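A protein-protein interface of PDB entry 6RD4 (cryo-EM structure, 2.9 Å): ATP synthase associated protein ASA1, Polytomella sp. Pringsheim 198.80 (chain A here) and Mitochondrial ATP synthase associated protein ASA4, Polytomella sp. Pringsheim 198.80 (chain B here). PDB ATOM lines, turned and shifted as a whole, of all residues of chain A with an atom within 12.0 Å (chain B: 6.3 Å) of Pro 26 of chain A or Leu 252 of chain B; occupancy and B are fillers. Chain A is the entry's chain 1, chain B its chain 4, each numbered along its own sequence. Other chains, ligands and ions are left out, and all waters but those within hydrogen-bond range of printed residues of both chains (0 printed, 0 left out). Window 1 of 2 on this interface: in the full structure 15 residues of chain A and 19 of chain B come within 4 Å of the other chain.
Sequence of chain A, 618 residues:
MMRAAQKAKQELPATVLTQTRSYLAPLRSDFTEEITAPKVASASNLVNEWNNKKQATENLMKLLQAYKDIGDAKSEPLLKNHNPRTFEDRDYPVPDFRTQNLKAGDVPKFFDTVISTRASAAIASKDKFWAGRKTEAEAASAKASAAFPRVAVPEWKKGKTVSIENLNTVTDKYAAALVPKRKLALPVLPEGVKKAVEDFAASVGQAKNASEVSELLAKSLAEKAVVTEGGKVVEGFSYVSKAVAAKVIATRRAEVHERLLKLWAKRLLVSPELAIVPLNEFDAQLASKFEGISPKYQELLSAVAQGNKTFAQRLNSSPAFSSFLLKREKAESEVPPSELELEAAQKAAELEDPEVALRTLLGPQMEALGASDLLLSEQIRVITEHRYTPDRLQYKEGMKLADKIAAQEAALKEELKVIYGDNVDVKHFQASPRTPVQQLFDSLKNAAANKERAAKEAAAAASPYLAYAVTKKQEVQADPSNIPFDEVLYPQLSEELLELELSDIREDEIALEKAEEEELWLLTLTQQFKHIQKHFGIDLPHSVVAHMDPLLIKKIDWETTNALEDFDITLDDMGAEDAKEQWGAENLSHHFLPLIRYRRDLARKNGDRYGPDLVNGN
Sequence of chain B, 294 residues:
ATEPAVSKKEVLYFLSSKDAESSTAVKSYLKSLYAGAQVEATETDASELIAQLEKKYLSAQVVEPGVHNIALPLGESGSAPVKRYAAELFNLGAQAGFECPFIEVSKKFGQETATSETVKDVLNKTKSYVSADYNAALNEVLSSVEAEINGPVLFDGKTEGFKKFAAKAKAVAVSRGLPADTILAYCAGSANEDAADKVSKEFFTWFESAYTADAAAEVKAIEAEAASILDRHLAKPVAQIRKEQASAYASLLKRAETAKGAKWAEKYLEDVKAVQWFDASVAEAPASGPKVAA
Of the 8 printed residues of chain A, 5 touch a printed residue of chain B.
Printed residues of chain A that touch a printed residue of chain B: Tyr 23, Leu 24, Ala 25, Pro 26 and Leu 27.
Hydrophobic or aromatic side chains of chain A that line the printed part of chain B: Tyr 23, Leu 24 and Leu 27.
Of the 13 printed residues of chain B, 3 touch a printed residue of chain A.
Among the printed residues, 8 pairs touch across the chains.
Among the printed residues, merely in contact across the chains: Leu 24 of chain A with Tyr 249 of chain B (3.6 Å), Leu 24 of chain A with Leu 252 of chain B (3.6 Å), Leu 24 of chain A with Tyr 268 of chain B (3.6 Å), Ala 25 of chain A with Leu 252 of chain B (3.8 Å), Pro 26 of chain A with Leu 252 of chain B (3.8 Å) and Leu 27 of chain A with Tyr 268 of chain B (3.6 Å).
The side-chain hydroxyl of Tyr 23 of chain A lies within hydrogen-bond range of the side-chain hydroxyl of Tyr 249 of chain B (3.5 Å).
OH of Tyr 268 of chain B sits at hydrogen-bond distance from O of Ala 25 of chain A (2.5 Å).
Pro 26 of chain A touches just one residue of chain B: Leu 252.
Leu 252 of chain B touches just these residues of chain A: Leu 24, Ala 25 and Pro 26.
No residue of chain A comes within 4 Å of Ala 250 of chain B.
No residue of chain A comes within 4 Å of Leu 253 of chain B.
No residue of chain A comes within 4 Å of Arg 255 of chain B.
Of the printed residues of chain B, Leu 24 of chain A touches Tyr 249 (3.6 Å), Leu 252 (3.6 Å) and Tyr 268 (3.6 Å).
Of the printed residues of chain B, Ala 25 of chain A touches Leu 252 and Tyr 268.
Printed residues of chain A within 4 Å of Tyr 268 of chain B: Leu 24, Ala 25 and Leu 27.
Of the printed residues of chain B, Leu 27 of chain A touches Tyr 268.
Of the printed residues of chain A, Tyr 249 of chain B touches Tyr 23 and Leu 24.
The nearest printed residue of chain A that does not touch Tyr 249 of chain B is Ala 25 of chain A (7.5 Å).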
ATOM      1  N   TYR A  23     -28.666  -1.349   5.396  1.00  0.00           N
ATOM      2  CA  TYR A  23     -29.632  -2.279   4.850  1.00  0.00           C
ATOM      3  C   TYR A  23     -28.943  -3.531   4.389  1.00  0.00           C
ATOM      4  O   TYR A  23     -29.581  -4.527   4.098  1.00  0.00           O
ATOM      5  CB  TYR A  23     -30.399  -1.654   3.693  1.00  0.00           C
ATOM      6  CG  TYR A  23     -29.546  -1.002   2.637  1.00  0.00           C
ATOM      7  CD1 TYR A  23     -29.310   0.354   2.667  1.00  0.00           C
ATOM      8  CD2 TYR A  23     -29.002  -1.737   1.600  1.00  0.00           C
ATOM      9  CE1 TYR A  23     -28.551   0.954   1.715  1.00  0.00           C
ATOM     10  CE2 TYR A  23     -28.239  -1.145   0.648  1.00  0.00           C
ATOM     11  CZ  TYR A  23     -28.017   0.202   0.712  1.00  0.00           C
ATOM     12  OH  TYR A  23     -27.255   0.813  -0.243  1.00  0.00           O
ATOM     13  N   LEU A  24     -27.631  -3.468   4.285  1.00  0.00           N
ATOM     14  CA  LEU A  24     -26.856  -4.570   3.748  1.00  0.00           C
ATOM     15  C   LEU A  24     -26.308  -5.467   4.847  1.00  0.00           C
ATOM     16  O   LEU A  24     -26.075  -5.037   5.977  1.00  0.00           O
ATOM     17  CB  LEU A  24     -25.745  -4.039   2.845  1.00  0.00           C
ATOM     18  CG  LEU A  24     -25.097  -2.705   3.163  1.00  0.00           C
ATOM     19  CD1 LEU A  24     -24.181  -2.808   4.286  1.00  0.00           C
ATOM     20  CD2 LEU A  24     -24.331  -2.291   1.954  1.00  0.00           C
ATOM     21  N   ALA A  25     -26.113  -6.722   4.495  1.00  0.00           N
ATOM     22  CA  ALA A  25     -25.840  -7.797   5.421  1.00  0.00           C
ATOM     23  C   ALA A  25     -24.420  -8.310   5.256  1.00  0.00           C
ATOM     24  O   ALA A  25     -23.799  -8.117   4.207  1.00  0.00           O
ATOM     25  CB  ALA A  25     -26.836  -8.940   5.185  1.00  0.00           C
ATOM     26  N   PRO A  26     -23.856  -8.948   6.279  1.00  0.00           N
ATOM     27  CA  PRO A  26     -22.598  -9.670   6.080  1.00  0.00           C
ATOM     28  C   PRO A  26     -22.821 -10.911   5.236  1.00  0.00           C
ATOM     29  O   PRO A  26     -23.752 -11.681   5.471  1.00  0.00           O
ATOM     30  CB  PRO A  26     -22.164 -10.026   7.502  1.00  0.00           C
ATOM     31  CG  PRO A  26     -23.389  -9.959   8.294  1.00  0.00           C
ATOM     32  CD  PRO A  26     -24.211  -8.878   7.702  1.00  0.00           C
ATOM     33  N   LEU A  27     -21.965 -11.099   4.243  1.00  0.00           N
ATOM     34  CA  LEU A  27     -22.056 -12.269   3.392  1.00  0.00           C
ATOM     35  C   LEU A  27     -21.422 -13.463   4.085  1.00  0.00           C
ATOM     36  O   LEU A  27     -20.320 -13.365   4.626  1.00  0.00           O
ATOM     37  CB  LEU A  27     -21.372 -12.007   2.056  1.00  0.00           C
ATOM     38  CG  LEU A  27     -22.028 -11.045   1.080  1.00  0.00           C
ATOM     39  CD1 LEU A  27     -21.373 -11.163  -0.264  1.00  0.00           C
ATOM     40  CD2 LEU A  27     -23.497 -11.316   0.970  1.00  0.00           C
ATOM     41  N   ARG A  28     -22.120 -14.591   4.075  1.00  0.00           N
ATOM     42  CA  ARG A  28     -21.651 -15.805   4.719  1.00  0.00           C
ATOM     43  C   ARG A  28     -21.672 -16.943   3.718  1.00  0.00           C
ATOM     44  O   ARG A  28     -22.574 -17.030   2.884  1.00  0.00           O
ATOM     45  CB  ARG A  28     -22.509 -16.157   5.924  1.00  0.00           C
ATOM     46  CG  ARG A  28     -22.360 -15.185   7.058  1.00  0.00           C
ATOM     47  CD  ARG A  28     -23.423 -15.374   8.101  1.00  0.00           C
ATOM     48  NE  ARG A  28     -23.566 -16.770   8.476  1.00  0.00           N
ATOM     49  CZ  ARG A  28     -24.305 -17.183   9.490  1.00  0.00           C
ATOM     50  NH1 ARG A  28     -24.390 -18.470   9.768  1.00  0.00           N
ATOM     51  NH2 ARG A  28     -24.952 -16.304  10.228  1.00  0.00           N
ATOM     52  N   SER A  29     -20.667 -17.806   3.795  1.00  0.00           N
ATOM     53  CA  SER A  29     -20.558 -18.972   2.929  1.00  0.00           C
ATOM     54  C   SER A  29     -20.256 -20.162   3.821  1.00  0.00           C
ATOM     55  O   SER A  29     -19.105 -20.585   3.931  1.00  0.00           O
ATOM     56  CB  SER A  29     -19.483 -18.773   1.894  1.00  0.00           C
ATOM     57  OG  SER A  29     -18.212 -18.718   2.507  1.00  0.00           O
ATOM     58  N   ASP A  30     -21.288 -20.707   4.447  1.00  0.00           N
ATOM     59  CA  ASP A  30     -21.133 -21.863   5.307  1.00  0.00           C
ATOM     60  C   ASP A  30     -22.435 -22.634   5.300  1.00  0.00           C
ATOM     61  O   ASP A  30     -23.497 -22.085   5.010  1.00  0.00           O
ATOM     62  CB  ASP A  30     -20.761 -21.483   6.735  1.00  0.00           C
ATOM     63  CG  ASP A  30     -21.861 -20.746   7.444  1.00  0.00           C
ATOM     64  OD1 ASP A  30     -22.222 -19.656   6.981  1.00  0.00           O
ATOM     65  OD2 ASP A  30     -22.384 -21.257   8.452  1.00  0.00           O
ATOM     66  N   SER B 247     -22.876   3.178  11.638  1.00  0.00           N
ATOM     67  CA  SER B 247     -21.622   2.500  11.927  1.00  0.00           C
ATOM     68  C   SER B 247     -21.596   1.114  11.315  1.00  0.00           C
ATOM     69  O   SER B 247     -20.560   0.673  10.812  1.00  0.00           O
ATOM     70  CB  SER B 247     -21.408   2.397  13.428  1.00  0.00           C
ATOM     71  OG  SER B 247     -20.292   1.579  13.711  1.00  0.00           O
ATOM     72  N   ALA B 248     -22.721   0.409  11.357  1.00  0.00           N
ATOM     73  CA  ALA B 248     -22.772  -0.929  10.795  1.00  0.00           C
ATOM     74  C   ALA B 248     -22.837  -0.903   9.282  1.00  0.00           C
ATOM     75  O   ALA B 248     -22.356  -1.829   8.634  1.00  0.00           O
ATOM     76  CB  ALA B 248     -23.964  -1.694  11.359  1.00  0.00           C
ATOM     77  N   TYR B 249     -23.423   0.136   8.701  1.00  0.00           N
ATOM     78  CA  TYR B 249     -23.456   0.226   7.251  1.00  0.00           C
ATOM     79  C   TYR B 249     -22.100   0.588   6.692  1.00  0.00           C
ATOM     80  O   TYR B 249     -21.711   0.077   5.643  1.00  0.00           O
ATOM     81  CB  TYR B 249     -24.485   1.258   6.817  1.00  0.00           C
ATOM     82  CG  TYR B 249     -24.502   1.560   5.344  1.00  0.00           C
ATOM     83  CD1 TYR B 249     -25.136   0.718   4.459  1.00  0.00           C
ATOM     84  CD2 TYR B 249     -23.913   2.703   4.847  1.00  0.00           C
ATOM     85  CE1 TYR B 249     -25.164   0.997   3.123  1.00  0.00           C
ATOM     86  CE2 TYR B 249     -23.934   2.981   3.517  1.00  0.00           C
ATOM     87  CZ  TYR B 249     -24.559   2.126   2.659  1.00  0.00           C
ATOM     88  OH  TYR B 249     -24.584   2.410   1.320  1.00  0.00           O
ATOM     89  N   ALA B 250     -21.375   1.477   7.362  1.00  0.00           N
ATOM     90  CA  ALA B 250     -20.107   1.944   6.829  1.00  0.00           C
ATOM     91  C   ALA B 250     -19.001   0.933   7.044  1.00  0.00           C
ATOM     92  O   ALA B 250     -18.076   0.858   6.233  1.00  0.00           O
ATOM     93  CB  ALA B 250     -19.734   3.275   7.466  1.00  0.00           C
ATOM     94  N   SER B 251     -19.080   0.158   8.123  1.00  0.00           N
ATOM     95  CA  SER B 251     -18.114  -0.907   8.351  1.00  0.00           C
ATOM     96  C   SER B 251     -18.270  -2.018   7.331  1.00  0.00           C
ATOM     97  O   SER B 251     -17.292  -2.669   6.956  1.00  0.00           O
ATOM     98  CB  SER B 251     -18.280  -1.467   9.757  1.00  0.00           C
ATOM     99  OG  SER B 251     -17.438  -2.582   9.960  1.00  0.00           O
ATOM    100  N   LEU B 252     -19.491  -2.252   6.876  1.00  0.00           N
ATOM    101  CA  LEU B 252     -19.750  -3.294   5.901  1.00  0.00           C
ATOM    102  C   LEU B 252     -19.452  -2.848   4.481  1.00  0.00           C
ATOM    103  O   LEU B 252     -19.271  -3.703   3.613  1.00  0.00           O
ATOM    104  CB  LEU B 252     -21.198  -3.743   6.005  1.00  0.00           C
ATOM    105  CG  LEU B 252     -21.670  -4.927   6.833  1.00  0.00           C
ATOM    106  CD1 LEU B 252     -21.214  -6.182   6.165  1.00  0.00           C
ATOM    107  CD2 LEU B 252     -21.165  -4.872   8.244  1.00  0.00           C
ATOM    108  N   LEU B 253     -19.422  -1.543   4.213  1.00  0.00           N
ATOM    109  CA  LEU B 253     -18.962  -1.081   2.908  1.00  0.00           C
ATOM    110  C   LEU B 253     -17.466  -1.244   2.760  1.00  0.00           C
ATOM    111  O   LEU B 253     -16.988  -1.680   1.706  1.00  0.00           O
ATOM    112  CB  LEU B 253     -19.315   0.381   2.679  1.00  0.00           C
ATOM    113  CG  LEU B 253     -20.640   0.701   2.031  1.00  0.00           C
ATOM    114  CD1 LEU B 253     -20.772   2.184   1.893  1.00  0.00           C
ATOM    115  CD2 LEU B 253     -20.626   0.077   0.687  1.00  0.00           C
ATOM    116  N   LYS B 254     -16.704  -0.890   3.792  1.00  0.00           N
ATOM    117  CA  LYS B 254     -15.257  -0.956   3.661  1.00  0.00           C
ATOM    118  C   LYS B 254     -14.758  -2.386   3.722  1.00  0.00           C
ATOM    119  O   LYS B 254     -13.624  -2.655   3.323  1.00  0.00           O
ATOM    120  CB  LYS B 254     -14.580  -0.092   4.717  1.00  0.00           C
ATOM    121  CG  LYS B 254     -14.771  -0.533   6.138  1.00  0.00           C
ATOM    122  CD  LYS B 254     -14.027   0.424   7.052  1.00  0.00           C
ATOM    123  CE  LYS B 254     -14.703   1.793   7.049  1.00  0.00           C
ATOM    124  NZ  LYS B 254     -14.096   2.749   8.015  1.00  0.00           N
ATOM    125  N   ARG B 255     -15.574  -3.319   4.203  1.00  0.00           N
ATOM    126  CA  ARG B 255     -15.222  -4.719   4.026  1.00  0.00           C
ATOM    127  C   ARG B 255     -15.387  -5.146   2.577  1.00  0.00           C
ATOM    128  O   ARG B 255     -14.751  -6.108   2.137  1.00  0.00           O
ATOM    129  CB  ARG B 255     -16.060  -5.605   4.938  1.00  0.00           C
ATOM    130  CG  ARG B 255     -15.405  -6.929   5.247  1.00  0.00           C
ATOM    131  CD  ARG B 255     -16.302  -7.812   6.068  1.00  0.00           C
ATOM    132  NE  ARG B 255     -16.825  -7.126   7.240  1.00  0.00           N
ATOM    133  CZ  ARG B 255     -17.733  -7.650   8.054  1.00  0.00           C
ATOM    134  NH1 ARG B 255     -18.168  -6.965   9.102  1.00  0.00           N
ATOM    135  NH2 ARG B 255     -18.213  -8.862   7.815  1.00  0.00           N
ATOM    136  N   ALA B 256     -16.231  -4.456   1.823  1.00  0.00           N
ATOM    137  CA  ALA B 256     -16.335  -4.700   0.395  1.00  0.00           C
ATOM    138  C   ALA B 256     -15.429  -3.802  -0.424  1.00  0.00           C
ATOM    139  O   ALA B 256     -15.205  -4.084  -1.602  1.00  0.00           O
ATOM    140  CB  ALA B 256     -17.776  -4.516  -0.075  1.00  0.00           C
ATOM    141  N   GLU B 257     -14.916  -2.725   0.158  1.00  0.00           N
ATOM    142  CA  GLU B 257     -14.032  -1.842  -0.586  1.00  0.00           C
ATOM    143  C   GLU B 257     -12.571  -2.205  -0.421  1.00  0.00           C
ATOM    144  O   GLU B 257     -11.791  -2.038  -1.363  1.00  0.00           O
ATOM    145  CB  GLU B 257     -14.255  -0.392  -0.167  1.00  0.00           C
ATOM    146  CG  GLU B 257     -15.488   0.209  -0.794  1.00  0.00           C
ATOM    147  CD  GLU B 257     -15.883   1.511  -0.158  1.00  0.00           C
ATOM    148  OE1 GLU B 257     -15.333   1.838   0.912  1.00  0.00           O
ATOM    149  OE2 GLU B 257     -16.749   2.207  -0.719  1.00  0.00           O
ATOM    150  N   TYR B 268     -21.051  -6.823  -4.712  1.00  0.00           N
ATOM    151  CA  TYR B 268     -21.599  -6.148  -3.540  1.00  0.00           C
ATOM    152  C   TYR B 268     -21.820  -4.673  -3.816  1.00  0.00           C
ATOM    153  O   TYR B 268     -22.911  -4.146  -3.594  1.00  0.00           O
ATOM    154  CB  TYR B 268     -20.651  -6.314  -2.364  1.00  0.00           C
ATOM    155  CG  TYR B 268     -21.285  -6.296  -1.009  1.00  0.00           C
ATOM    156  CD1 TYR B 268     -21.358  -5.131  -0.275  1.00  0.00           C
ATOM    157  CD2 TYR B 268     -21.775  -7.454  -0.448  1.00  0.00           C
ATOM    158  CE1 TYR B 268     -21.920  -5.118   0.970  1.00  0.00           C
ATOM    159  CE2 TYR B 268     -22.339  -7.446   0.794  1.00  0.00           C
ATOM    160  CZ  TYR B 268     -22.407  -6.281   1.496  1.00  0.00           C
ATOM    161  OH  TYR B 268     -22.975  -6.299   2.735  1.00  0.00           O
ATOM    162  N   LEU B 269     -20.795  -3.991  -4.310  1.00  0.00           N
ATOM    163  CA  LEU B 269     -20.886  -2.569  -4.580  1.00  0.00           C
ATOM    164  C   LEU B 269     -21.653  -2.256  -5.850  1.00  0.00           C
ATOM    165  O   LEU B 269     -21.977  -1.092  -6.083  1.00  0.00           O
ATOM    166  CB  LEU B 269     -19.488  -1.976  -4.668  1.00  0.00           C
ATOM    167  CG  LEU B 269     -18.610  -2.294  -3.469  1.00  0.00           C
ATOM    168  CD1 LEU B 269     -17.238  -1.745  -3.690  1.00  0.00           C
ATOM    169  CD2 LEU B 269     -19.208  -1.696  -2.241  1.00  0.00           C
